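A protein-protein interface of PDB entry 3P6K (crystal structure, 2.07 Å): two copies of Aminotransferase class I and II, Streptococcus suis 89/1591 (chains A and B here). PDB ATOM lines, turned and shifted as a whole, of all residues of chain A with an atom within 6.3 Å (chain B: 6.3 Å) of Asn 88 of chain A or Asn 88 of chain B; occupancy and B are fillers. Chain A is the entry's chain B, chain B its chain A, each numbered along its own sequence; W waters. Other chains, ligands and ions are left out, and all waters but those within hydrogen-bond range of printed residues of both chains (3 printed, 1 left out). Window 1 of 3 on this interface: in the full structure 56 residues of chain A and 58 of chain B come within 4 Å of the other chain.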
ATOM      1  N   GLN A  86     -20.793 -12.274   8.308  1.00  0.00           N
ATOM      2  CA  GLN A  86     -19.864 -13.120   7.537  1.00  0.00           C
ATOM      3  C   GLN A  86     -20.314 -14.585   7.574  1.00  0.00           C
ATOM      4  O   GLN A  86     -20.868 -15.049   8.548  1.00  0.00           O
ATOM      5  CB  GLN A  86     -18.468 -13.013   8.102  1.00  0.00           C
ATOM      6  CG  GLN A  86     -17.365 -13.690   7.284  1.00  0.00           C
ATOM      7  CD  GLN A  86     -16.028 -13.376   7.870  1.00  0.00           C
ATOM      8  OE1 GLN A  86     -15.629 -13.975   8.874  1.00  0.00           O
ATOM      9  NE2 GLN A  86     -15.311 -12.435   7.257  1.00  0.00           N
ATOM     10  N   THR A  87     -20.093 -15.288   6.477  1.00  0.00           N
ATOM     11  CA  THR A  87     -20.456 -16.704   6.343  1.00  0.00           C
ATOM     12  C   THR A  87     -19.364 -17.475   5.597  1.00  0.00           C
ATOM     13  O   THR A  87     -18.439 -16.866   5.024  1.00  0.00           O
ATOM     14  CB  THR A  87     -21.794 -16.854   5.582  1.00  0.00           C
ATOM     15  OG1 THR A  87     -21.656 -16.276   4.273  1.00  0.00           O
ATOM     16  CG2 THR A  87     -22.937 -16.174   6.336  1.00  0.00           C
ATOM     17  N   ASN A  88     -19.436 -18.804   5.683  1.00  0.00           N
ATOM     18  CA  ASN A  88     -18.534 -19.715   4.944  1.00  0.00           C
ATOM     19  C   ASN A  88     -19.013 -19.797   3.490  1.00  0.00           C
ATOM     20  O   ASN A  88     -19.747 -20.722   3.080  1.00  0.00           O
ATOM     21  CB  ASN A  88     -18.372 -21.093   5.616  1.00  0.00           C
ATOM     22  CG  ASN A  88     -19.640 -21.907   5.657  1.00  0.00           C
ATOM     23  OD1 ASN A  88     -20.698 -21.421   6.062  1.00  0.00           O
ATOM     24  ND2 ASN A  88     -19.539 -23.159   5.224  1.00  0.00           N
ATOM     25  N   GLY A  89     -18.660 -18.761   2.731  1.00  0.00           N
ATOM     26  CA  GLY A  89     -19.121 -18.602   1.369  1.00  0.00           C
ATOM     27  C   GLY A  89     -20.607 -18.236   1.269  1.00  0.00           C
ATOM     28  O   GLY A  89     -21.325 -18.170   2.263  1.00  0.00           O
ATOM     29  N   ALA A  90     -21.060 -17.994   0.054  1.00  0.00           N
ATOM     30  CA  ALA A  90     -22.492 -17.803  -0.230  1.00  0.00           C
ATOM     31  C   ALA A  90     -23.250 -19.104   0.092  1.00  0.00           C
ATOM     32  O   ALA A  90     -24.403 -19.048   0.445  1.00  0.00           O
ATOM     33  CB  ALA A  90     -22.711 -17.397  -1.676  1.00  0.00           C
ATOM     34  N   THR A  91     -22.586 -20.267  -0.013  1.00  0.00           N
ATOM     35  CA  THR A  91     -23.175 -21.557   0.395  1.00  0.00           C
ATOM     36  C   THR A  91     -23.705 -21.493   1.815  1.00  0.00           C
ATOM     37  O   THR A  91     -24.864 -21.838   2.088  1.00  0.00           O
ATOM     38  CB  THR A  91     -22.177 -22.734   0.294  1.00  0.00           C
ATOM     39  OG1 THR A  91     -21.672 -22.832  -1.053  1.00  0.00           O
ATOM     40  CG2 THR A  91     -22.871 -24.087   0.652  1.00  0.00           C
ATOM     41  N   GLY A  92     -22.839 -21.067   2.718  1.00  0.00           N
ATOM     42  CA  GLY A  92     -23.191 -20.907   4.124  1.00  0.00           C
ATOM     43  C   GLY A  92     -24.258 -19.865   4.372  1.00  0.00           C
ATOM     44  O   GLY A  92     -25.125 -20.062   5.211  1.00  0.00           O
ATOM     45  N   ALA A  93     -24.217 -18.789   3.592  1.00  0.00           N
ATOM     46  CA  ALA A  93     -25.175 -17.689   3.711  1.00  0.00           C
ATOM     47  C   ALA A  93     -26.579 -18.106   3.267  1.00  0.00           C
ATOM     48  O   ALA A  93     -27.544 -17.865   4.002  1.00  0.00           O
ATOM     49  CB  ALA A  93     -24.687 -16.451   2.958  1.00  0.00           C
ATOM     50  N1  LLP A 222     -24.549 -19.602  -5.392  1.00  0.00           N
ATOM     51  C2  LLP A 222     -24.356 -19.731  -6.771  1.00  0.00           C
ATOM     52  C2' LLP A 222     -25.435 -19.276  -7.723  1.00  0.00           C
ATOM     53  C3  LLP A 222     -23.171 -20.304  -7.274  1.00  0.00           C
ATOM     54  O3  LLP A 222     -22.982 -20.467  -8.494  1.00  0.00           O
ATOM     55  C4  LLP A 222     -22.183 -20.721  -6.378  1.00  0.00           C
ATOM     56  C4' LLP A 222     -20.933 -21.314  -6.980  1.00  0.00           C
ATOM     57  C5  LLP A 222     -22.376 -20.585  -4.982  1.00  0.00           C
ATOM     58  C6  LLP A 222     -23.569 -20.017  -4.507  1.00  0.00           C
ATOM     59  C5' LLP A 222     -21.333 -20.998  -3.976  1.00  0.00           C
ATOM     60  OP4 LLP A 222     -20.431 -19.903  -3.619  1.00  0.00           O
ATOM     61  P   LLP A 222     -19.412 -19.979  -2.395  1.00  0.00           P
ATOM     62  OP1 LLP A 222     -19.231 -18.539  -2.101  1.00  0.00           O
ATOM     63  OP2 LLP A 222     -20.049 -20.785  -1.308  1.00  0.00           O
ATOM     64  OP3 LLP A 222     -18.230 -20.605  -2.987  1.00  0.00           O
ATOM     65  N   LLP A 222     -16.885 -16.058  -6.668  1.00  0.00           N
ATOM     66  CA  LLP A 222     -17.120 -15.972  -8.110  1.00  0.00           C
ATOM     67  CB  LLP A 222     -18.584 -16.190  -8.410  1.00  0.00           C
ATOM     68  CG  LLP A 222     -19.191 -17.475  -7.813  1.00  0.00           C
ATOM     69  CD  LLP A 222     -18.593 -18.743  -8.374  1.00  0.00           C
ATOM     70  CE  LLP A 222     -19.609 -19.924  -8.352  1.00  0.00           C
ATOM     71  NZ  LLP A 222     -19.959 -20.382  -7.022  1.00  0.00           N
ATOM     72  C   LLP A 222     -16.678 -14.648  -8.702  1.00  0.00           C
ATOM     73  O   LLP A 222     -15.851 -14.638  -9.595  1.00  0.00           O
ATOM     74  N   ARG A 230     -13.347 -19.354   1.369  1.00  0.00           N
ATOM     75  CA  ARG A 230     -14.725 -19.634   1.809  1.00  0.00           C
ATOM     76  C   ARG A 230     -15.287 -18.452   2.650  1.00  0.00           C
ATOM     77  O   ARG A 230     -15.547 -18.594   3.834  1.00  0.00           O
ATOM     78  CB  ARG A 230     -14.787 -20.937   2.610  1.00  0.00           C
ATOM     79  CG  ARG A 230     -14.029 -22.146   2.081  1.00  0.00           C
ATOM     80  CD  ARG A 230     -14.425 -22.628   0.728  1.00  0.00           C
ATOM     81  NE  ARG A 230     -15.849 -22.848   0.568  1.00  0.00           N
ATOM     82  CZ  ARG A 230     -16.678 -22.182  -0.237  1.00  0.00           C
ATOM     83  NH1 ARG A 230     -16.267 -21.178  -1.049  1.00  0.00           N
ATOM     84  NH2 ARG A 230     -17.955 -22.527  -0.224  1.00  0.00           N
ATOM     85  N   ILE A 231     -15.401 -17.291   2.027  1.00  0.00           N
ATOM     86  CA  ILE A 231     -15.890 -16.074   2.664  1.00  0.00           C
ATOM     87  C   ILE A 231     -17.015 -15.512   1.831  1.00  0.00           C
ATOM     88  O   ILE A 231     -16.836 -15.177   0.675  1.00  0.00           O
ATOM     89  CB  ILE A 231     -14.815 -14.976   2.841  1.00  0.00           C
ATOM     90  CG1 ILE A 231     -13.731 -15.424   3.832  1.00  0.00           C
ATOM     91  CG2 ILE A 231     -15.440 -13.669   3.330  1.00  0.00           C
ATOM     92  CD1 ILE A 231     -14.134 -15.430   5.321  1.00  0.00           C
ATOM     93  N   GLY A 232     -18.172 -15.431   2.463  1.00  0.00           N
ATOM     94  CA  GLY A 232     -19.322 -14.741   1.916  1.00  0.00           C
ATOM     95  C   GLY A 232     -19.974 -13.926   3.020  1.00  0.00           C
ATOM     96  O   GLY A 232     -19.418 -13.740   4.111  1.00  0.00           O
ATOM     97  N   ARG A 248     -26.181 -19.175  13.767  1.00  0.00           N
ATOM     98  CA  ARG A 248     -24.866 -19.464  13.133  1.00  0.00           C
ATOM     99  C   ARG A 248     -24.084 -20.696  13.620  1.00  0.00           C
ATOM    100  O   ARG A 248     -23.422 -21.379  12.813  1.00  0.00           O
ATOM    101  CB  ARG A 248     -23.993 -18.181  13.029  1.00  0.00           C
ATOM    102  CG  ARG A 248     -24.666 -17.202  12.083  1.00  0.00           C
ATOM    103  CD  ARG A 248     -24.020 -15.859  11.875  1.00  0.00           C
ATOM    104  NE  ARG A 248     -22.717 -15.940  11.216  1.00  0.00           N
ATOM    105  CZ  ARG A 248     -21.536 -15.967  11.834  1.00  0.00           C
ATOM    106  NH1 ARG A 248     -21.441 -15.908  13.177  1.00  0.00           N
ATOM    107  NH2 ARG A 248     -20.421 -16.048  11.099  1.00  0.00           N
ATOM    108  N   THR A 251     -24.641 -24.134  11.715  1.00  0.00           N
ATOM    109  CA  THR A 251     -24.104 -24.372  10.402  1.00  0.00           C
ATOM    110  C   THR A 251     -22.630 -24.144  10.202  1.00  0.00           C
ATOM    111  O   THR A 251     -21.999 -24.860   9.396  1.00  0.00           O
ATOM    112  CB  THR A 251     -24.897 -23.506   9.388  1.00  0.00           C
ATOM    113  OG1 THR A 251     -24.614 -22.095   9.581  1.00  0.00           O
ATOM    114  CG2 THR A 251     -26.457 -23.758   9.502  1.00  0.00           C
ATOM    115  N   MET A 252     -22.085 -23.152  10.904  1.00  0.00           N
ATOM    116  CA  MET A 252     -20.685 -22.793  10.741  1.00  0.00           C
ATOM    117  C   MET A 252     -19.897 -22.295  11.947  1.00  0.00           C
ATOM    118  O   MET A 252     -18.665 -22.398  11.920  1.00  0.00           O
ATOM    119  CB  MET A 252     -20.667 -21.659   9.714  1.00  0.00           C
ATOM    120  CG  MET A 252     -21.389 -20.389  10.236  1.00  0.00           C
ATOM    121  SD  MET A 252     -21.327 -19.017   8.968  1.00  0.00           S
ATOM    122  CE  MET A 252     -22.691 -19.753   7.805  1.00  0.00           C
ATOM    123  N   CYS A 254     -18.403 -19.757  12.571  1.00  0.00           N
ATOM    124  CA  CYS A 254     -17.754 -18.662  11.901  1.00  0.00           C
ATOM    125  C   CYS A 254     -16.902 -19.181  10.775  1.00  0.00           C
ATOM    126  O   CYS A 254     -16.659 -20.404  10.666  1.00  0.00           O
ATOM    127  CB  CYS A 254     -16.847 -17.906  12.904  1.00  0.00           C
ATOM    128  SG  CYS A 254     -15.699 -18.955  13.769  1.00  0.00           S
ATOM    129  N   ALA A 255     -16.415 -18.233   9.983  1.00  0.00           N
ATOM    130  CA  ALA A 255     -15.479 -18.478   8.895  1.00  0.00           C
ATOM    131  C   ALA A 255     -14.089 -18.372   9.522  1.00  0.00           C
ATOM    132  O   ALA A 255     -13.958 -18.063  10.694  1.00  0.00           O
ATOM    133  CB  ALA A 255     -15.687 -17.445   7.790  1.00  0.00           C
ATOM    134  N   GLN B  86     -13.133 -34.158   4.718  1.00  0.00           N
ATOM    135  CA  GLN B  86     -12.860 -32.885   5.376  1.00  0.00           C
ATOM    136  C   GLN B  86     -14.125 -32.015   5.430  1.00  0.00           C
ATOM    137  O   GLN B  86     -14.905 -31.975   4.488  1.00  0.00           O
ATOM    138  CB  GLN B  86     -11.781 -32.126   4.606  1.00  0.00           C
ATOM    139  CG  GLN B  86     -11.249 -30.896   5.336  1.00  0.00           C
ATOM    140  CD  GLN B  86     -10.080 -30.319   4.587  1.00  0.00           C
ATOM    141  OE1 GLN B  86     -10.280 -29.700   3.547  1.00  0.00           O
ATOM    142  NE2 GLN B  86      -8.857 -30.569   5.072  1.00  0.00           N
ATOM    143  N   THR B  87     -14.305 -31.302   6.536  1.00  0.00           N
ATOM    144  CA  THR B  87     -15.441 -30.390   6.737  1.00  0.00           C
ATOM    145  C   THR B  87     -14.973 -29.076   7.343  1.00  0.00           C
ATOM    146  O   THR B  87     -13.826 -28.967   7.783  1.00  0.00           O
ATOM    147  CB  THR B  87     -16.477 -31.023   7.680  1.00  0.00           C
ATOM    148  OG1 THR B  87     -15.895 -31.191   8.995  1.00  0.00           O
ATOM    149  CG2 THR B  87     -16.995 -32.394   7.129  1.00  0.00           C
ATOM    150  N   ASN B  88     -15.837 -28.075   7.290  1.00  0.00           N
ATOM    151  CA  ASN B  88     -15.604 -26.794   7.976  1.00  0.00           C
ATOM    152  C   ASN B  88     -15.891 -26.947   9.482  1.00  0.00           C
ATOM    153  O   ASN B  88     -16.957 -26.589   9.978  1.00  0.00           O
ATOM    154  CB  ASN B  88     -16.407 -25.624   7.378  1.00  0.00           C
ATOM    155  CG  ASN B  88     -17.909 -25.865   7.373  1.00  0.00           C
ATOM    156  OD1 ASN B  88     -18.358 -26.952   6.995  1.00  0.00           O
ATOM    157  ND2 ASN B  88     -18.678 -24.865   7.775  1.00  0.00           N
ATOM    158  N   GLY B  89     -14.921 -27.496  10.192  1.00  0.00           N
ATOM    159  CA  GLY B  89     -15.050 -27.813  11.619  1.00  0.00           C
ATOM    160  C   GLY B  89     -15.942 -29.022  11.895  1.00  0.00           C
ATOM    161  O   GLY B  89     -16.460 -29.645  10.966  1.00  0.00           O
ATOM    162  N   ALA B  90     -16.096 -29.372  13.173  1.00  0.00           N
ATOM    163  CA  ALA B  90     -17.038 -30.422  13.606  1.00  0.00           C
ATOM    164  C   ALA B  90     -18.480 -29.948  13.421  1.00  0.00           C
ATOM    165  O   ALA B  90     -19.395 -30.768  13.240  1.00  0.00           O
ATOM    166  CB  ALA B  90     -16.799 -30.798  15.063  1.00  0.00           C
ATOM    167  N   THR B  91     -18.680 -28.629  13.507  1.00  0.00           N
ATOM    168  CA  THR B  91     -19.981 -27.994  13.262  1.00  0.00           C
ATOM    169  C   THR B  91     -20.452 -28.326  11.874  1.00  0.00           C
ATOM    170  O   THR B  91     -21.591 -28.754  11.699  1.00  0.00           O
ATOM    171  CB  THR B  91     -19.938 -26.448  13.360  1.00  0.00           C
ATOM    172  OG1 THR B  91     -19.528 -26.071  14.667  1.00  0.00           O
ATOM    173  CG2 THR B  91     -21.345 -25.828  13.090  1.00  0.00           C
ATOM    174  N   GLY B  92     -19.566 -28.132  10.903  1.00  0.00           N
ATOM    175  CA  GLY B  92     -19.860 -28.451   9.535  1.00  0.00           C
ATOM    176  C   GLY B  92     -20.043 -29.934   9.291  1.00  0.00           C
ATOM    177  O   GLY B  92     -20.911 -30.309   8.511  1.00  0.00           O
ATOM    178  N   ALA B  93     -19.265 -30.776   9.980  1.00  0.00           N
ATOM    179  CA  ALA B  93     -19.383 -32.247   9.880  1.00  0.00           C
ATOM    180  C   ALA B  93     -20.740 -32.786  10.418  1.00  0.00           C
ATOM    181  O   ALA B  93     -21.411 -33.598   9.773  1.00  0.00           O
ATOM    182  CB  ALA B  93     -18.209 -32.910  10.602  1.00  0.00           C
ATOM    183  N1  LLP B 222     -19.091 -30.237  18.977  1.00  0.00           N
ATOM    184  C2  LLP B 222     -18.933 -29.923  20.339  1.00  0.00           C
ATOM    185  C2' LLP B 222     -19.368 -30.905  21.390  1.00  0.00           C
ATOM    186  C3  LLP B 222     -18.353 -28.702  20.726  1.00  0.00           C
ATOM    187  O3  LLP B 222     -18.217 -28.430  21.943  1.00  0.00           O
ATOM    188  C4  LLP B 222     -17.937 -27.784  19.726  1.00  0.00           C
ATOM    189  C4' LLP B 222     -17.297 -26.461  20.142  1.00  0.00           C
ATOM    190  C5  LLP B 222     -18.133 -28.107  18.354  1.00  0.00           C
ATOM    191  C6  LLP B 222     -18.701 -29.342  17.992  1.00  0.00           C
ATOM    192  C5' LLP B 222     -17.705 -27.186  17.247  1.00  0.00           C
ATOM    193  OP4 LLP B 222     -16.366 -27.476  16.771  1.00  0.00           O
ATOM    194  P   LLP B 222     -15.753 -26.796  15.514  1.00  0.00           P
ATOM    195  OP1 LLP B 222     -14.760 -27.787  15.030  1.00  0.00           O
ATOM    196  OP2 LLP B 222     -16.870 -26.521  14.540  1.00  0.00           O
ATOM    197  OP3 LLP B 222     -15.117 -25.539  15.942  1.00  0.00           O
ATOM    198  N   LLP B 222     -10.862 -28.041  19.242  1.00  0.00           N
ATOM    199  CA  LLP B 222     -10.844 -28.182  20.703  1.00  0.00           C
ATOM    200  CB  LLP B 222     -12.105 -28.923  21.186  1.00  0.00           C
ATOM    201  CG  LLP B 222     -13.461 -28.310  20.771  1.00  0.00           C
ATOM    202  CD  LLP B 222     -13.690 -26.877  21.277  1.00  0.00           C
ATOM    203  CE  LLP B 222     -15.188 -26.443  21.292  1.00  0.00           C
ATOM    204  NZ  LLP B 222     -15.941 -26.500  19.986  1.00  0.00           N
ATOM    205  C   LLP B 222      -9.583 -28.899  21.168  1.00  0.00           C
ATOM    206  O   LLP B 222      -8.831 -28.370  21.956  1.00  0.00           O
ATOM    207  N   ILE B 229      -8.955 -22.101  11.831  1.00  0.00           N
ATOM    208  CA  ILE B 229      -8.885 -22.665  10.473  1.00  0.00           C
ATOM    209  C   ILE B 229     -10.168 -23.386  10.039  1.00  0.00           C
ATOM    210  O   ILE B 229     -10.307 -23.700   8.860  1.00  0.00           O
ATOM    211  CB  ILE B 229      -7.641 -23.555  10.210  1.00  0.00           C
ATOM    212  CG1 ILE B 229      -7.620 -24.850  11.047  1.00  0.00           C
ATOM    213  CG2 ILE B 229      -6.350 -22.727  10.434  1.00  0.00           C
ATOM    214  CD1 ILE B 229      -6.439 -25.768  10.697  1.00  0.00           C
ATOM    215  N   ARG B 230     -11.101 -23.655  10.962  1.00  0.00           N
ATOM    216  CA  ARG B 230     -12.370 -24.309  10.632  1.00  0.00           C
ATOM    217  C   ARG B 230     -12.139 -25.621   9.862  1.00  0.00           C
ATOM    218  O   ARG B 230     -12.587 -25.797   8.711  1.00  0.00           O
ATOM    219  CB  ARG B 230     -13.304 -23.377   9.839  1.00  0.00           C
ATOM    220  CG  ARG B 230     -13.371 -21.930  10.294  1.00  0.00           C
ATOM    221  CD  ARG B 230     -13.819 -21.709  11.721  1.00  0.00           C
ATOM    222  NE  ARG B 230     -15.049 -22.432  12.081  1.00  0.00           N
ATOM    223  CZ  ARG B 230     -15.173 -23.405  12.992  1.00  0.00           C
ATOM    224  NH1 ARG B 230     -14.137 -23.842  13.758  1.00  0.00           N
ATOM    225  NH2 ARG B 230     -16.380 -23.942  13.179  1.00  0.00           N
ATOM    226  N   ILE B 231     -11.409 -26.532  10.495  1.00  0.00           N
ATOM    227  CA  ILE B 231     -11.118 -27.816   9.880  1.00  0.00           C
ATOM    228  C   ILE B 231     -11.537 -28.976  10.771  1.00  0.00           C
ATOM    229  O   ILE B 231     -11.045 -29.139  11.896  1.00  0.00           O
ATOM    230  CB  ILE B 231      -9.652 -27.981   9.512  1.00  0.00           C
ATOM    231  CG1 ILE B 231      -9.282 -27.082   8.321  1.00  0.00           C
ATOM    232  CG2 ILE B 231      -9.362 -29.456   9.091  1.00  0.00           C
ATOM    233  CD1 ILE B 231      -9.886 -27.498   6.945  1.00  0.00           C
ATOM    234  N   GLY B 232     -12.458 -29.771  10.228  1.00  0.00           N
ATOM    235  CA  GLY B 232     -12.922 -30.982  10.859  1.00  0.00           C
ATOM    236  C   GLY B 232     -13.013 -32.116   9.853  1.00  0.00           C
ATOM    237  O   GLY B 232     -12.574 -32.013   8.698  1.00  0.00           O
ATOM    238  N   THR B 251     -24.102 -27.335   2.231  1.00  0.00           N
ATOM    239  CA  THR B 251     -23.623 -26.837   3.530  1.00  0.00           C
ATOM    240  C   THR B 251     -22.327 -26.063   3.502  1.00  0.00           C
ATOM    241  O   THR B 251     -22.155 -25.119   4.298  1.00  0.00           O
ATOM    242  CB  THR B 251     -23.512 -28.029   4.547  1.00  0.00           C
ATOM    243  OG1 THR B 251     -22.421 -28.902   4.191  1.00  0.00           O
ATOM    244  CG2 THR B 251     -24.835 -28.843   4.594  1.00  0.00           C
ATOM    245  N   MET B 252     -21.417 -26.458   2.609  1.00  0.00           N
ATOM    246  CA  MET B 252     -20.122 -25.834   2.539  1.00  0.00           C
ATOM    247  C   MET B 252     -19.360 -25.836   1.223  1.00  0.00           C
ATOM    248  O   MET B 252     -18.482 -24.988   1.086  1.00  0.00           O
ATOM    249  CB  MET B 252     -19.213 -26.540   3.575  1.00  0.00           C
ATOM    250  CG  MET B 252     -19.087 -28.044   3.343  1.00  0.00           C
ATOM    251  SD  MET B 252     -17.517 -28.868   4.179  1.00  0.00           S
ATOM    252  CE  MET B 252     -17.864 -30.592   3.572  1.00  0.00           C
ATOM    253  N   ILE B 253     -19.663 -26.779   0.312  1.00  0.00           N
ATOM    254  CA  ILE B 253     -18.836 -27.138  -0.852  1.00  0.00           C
ATOM    255  C   ILE B 253     -17.524 -27.766  -0.365  1.00  0.00           C
ATOM    256  O   ILE B 253     -17.247 -28.933  -0.683  1.00  0.00           O
ATOM    257  CB  ILE B 253     -18.532 -26.009  -1.893  1.00  0.00           C
ATOM    258  CG1 ILE B 253     -19.843 -25.361  -2.363  1.00  0.00           C
ATOM    259  CG2 ILE B 253     -17.783 -26.631  -3.091  1.00  0.00           C
ATOM    260  CD1 ILE B 253     -19.642 -24.196  -3.360  1.00  0.00           C
ATOM    261  N   CYS B 254     -16.715 -26.996   0.377  1.00  0.00           N
ATOM    262  CA  CYS B 254     -15.451 -27.463   0.924  1.00  0.00           C
ATOM    263  C   CYS B 254     -14.899 -26.469   1.965  1.00  0.00           C
ATOM    264  O   CYS B 254     -15.422 -25.339   2.127  1.00  0.00           O
ATOM    265  CB  CYS B 254     -14.412 -27.627  -0.234  1.00  0.00           C
ATOM    266  SG  CYS B 254     -14.128 -26.073  -1.155  1.00  0.00           S
ATOM    267  N   ALA B 255     -13.845 -26.903   2.650  1.00  0.00           N
ATOM    268  CA  ALA B 255     -13.111 -26.067   3.599  1.00  0.00           C
ATOM    269  C   ALA B 255     -12.074 -25.278   2.806  1.00  0.00           C
ATOM    270  O   ALA B 255     -11.867 -25.504   1.610  1.00  0.00           O
ATOM    271  CB  ALA B 255     -12.438 -26.896   4.701  1.00  0.00           C
HETATM  272  O   HOH W   1     -16.768 -22.322   8.202  1.00  0.00           O
HETATM  273  O   HOH W   2     -21.338 -25.908   7.269  1.00  0.00           O
HETATM  274  O   HOH W   3     -16.429 -23.837   4.371  1.00  0.00           O
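The side-chain amide nitrogen of Asn 88 of chain B sits close to the side-chain amide nitrogen of Asn 88 of chain A. O of Met 252 of chain A sits at hydrogen-bond distance from NH2 of Arg 230 of chain B, 3.0 Å away. O of Cys 254 of chain A lies within hydrogen-bond range of NE of Arg 230 of chain B. The backbone carbonyl oxygen of Thr 251 of chain B sits at hydrogen-bond distance from the side-chain amide nitrogen of Asn 88 of chain A, at 3.4 Å. NH2 of Arg 230 of chain A sits at hydrogen-bond distance from O of Met 252 of chain B (2.8 Å). The backbone carbonyl oxygen (O) of Cys 254 of chain B lies within hydrogen-bond range of the guanidinium group (NE) of Arg 230 of chain A, 3.0 Å away.
Asn 88 of chain A touches Met 252 of chain B (ND2 to CB, 3.8 Å). Thr 91 of chain A touches Thr 251 of chain B. Met 252 of chain B touches Thr 91 of chain A. Thr 91 of chain A touches Ile 253 of chain B (OG1 to CD1, 3.4 Å). CD1 of Ile 253 of chain B touches C5' of LLP 222 of chain A, 3.7 Å away. Arg 230 of chain A touches Ile 253 of chain B (NH2 to CB, 3.9 Å). CG of Arg 230 of chain A touches C of Ala 255 of chain B, at 3.8 Å. O of Thr 251 of chain A touches ND2 of Asn 88 of chain B, 3.7 Å away. Met 252 of chain A touches Thr 91 of chain B (N to CG2, 3.5 Å). Ala 255 of chain A touches Arg 230 of chain B (C to CG, 3.7 Å).
Asn 88 of chain A touches just these residues of chain B: Asn 88, Thr 251 and Met 252. Printed residues of chain B within 4 Å of LLP 222 of chain A: Ile 253. Asn 88 of chain B touches just these residues of chain A: Asn 88 and Thr 251. Ile 229 of chain B touches none of the printed residues of chain A. Of the printed residues of chain A, Ala 255 of chain B touches Arg 230 (3.8 Å). The nearest printed residue of chain A that does not touch Ile 253 of chain B is Asn 88 of chain A (6.1 Å).
OD1 of Asn 88 of chain B sits close to SD of Met 252 of chain B (3.5 Å). The backbone NH (N) of Gly 89 of chain B is in hydrogen-bond range of the backbone carbonyl oxygen (O) of Arg 230 of chain B. OP3 of LLP 222 of chain B sits close to NH1 of Arg 230 of chain B. The backbone carbonyl oxygen of Arg 230 of chain A sits at hydrogen-bond distance from the backbone NH of Gly 89 of chain A. OP1 of LLP 222 of chain A lies close to the backbone NH (N) of Ala 90 of chain A (2.9 Å). OP3 of LLP 222 of chain A sits close to the guanidinium group (NH1) of Arg 230 of chain A (2.8 Å).
Of the 17 printed residues of chain A, 8 touch a printed residue of chain B. Among the printed residues, 17 pairs touch across the chains.
Water W2 lies within hydrogen-bond range of O of Thr 251 of chain A (2.5 Å), ND2 of Asn 88 of chain B (2.9 Å) and O of Thr 251 of chain B (3.2 Å). Water W3 lies within hydrogen-bond range of the backbone carbonyl oxygen (O) of Cys 254 of chain B (2.9 Å) and the side-chain amide nitrogen (ND2) of Asn 88 of chain A (3.3 Å). Water W1 lies within hydrogen-bond range of the backbone carbonyl oxygen of Cys 254 of chain A and the side-chain amide nitrogen of Asn 88 of chain B.
Asn 88 of chain A touches Thr 251 of chain B, and with the chains exchanged Thr 251 of chain A touches Asn 88 of chain B. Thr 91 of chain A touches Met 252 of chain B, and with the chains exchanged Met 252 of chain A touches Thr 91 of chain B. Arg 230 of chain A touches Met 252 of chain B, and with the chains exchanged Met 252 of chain A touches Arg 230 of chain B. Arg 230 of chain A touches Ala 255 of chain B, and with the chains exchanged Ala 255 of chain A touches Arg 230 of chain B. Positions printed for both chains: 86, 87, 88, 89, 90, 91, 92, 93, 222, 230, 231, 232, 251, 252, 254 and 255. Of the 17 pairs that touch across the chains among the printed residues, 13 have their exchanged pair printed and touching as well.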
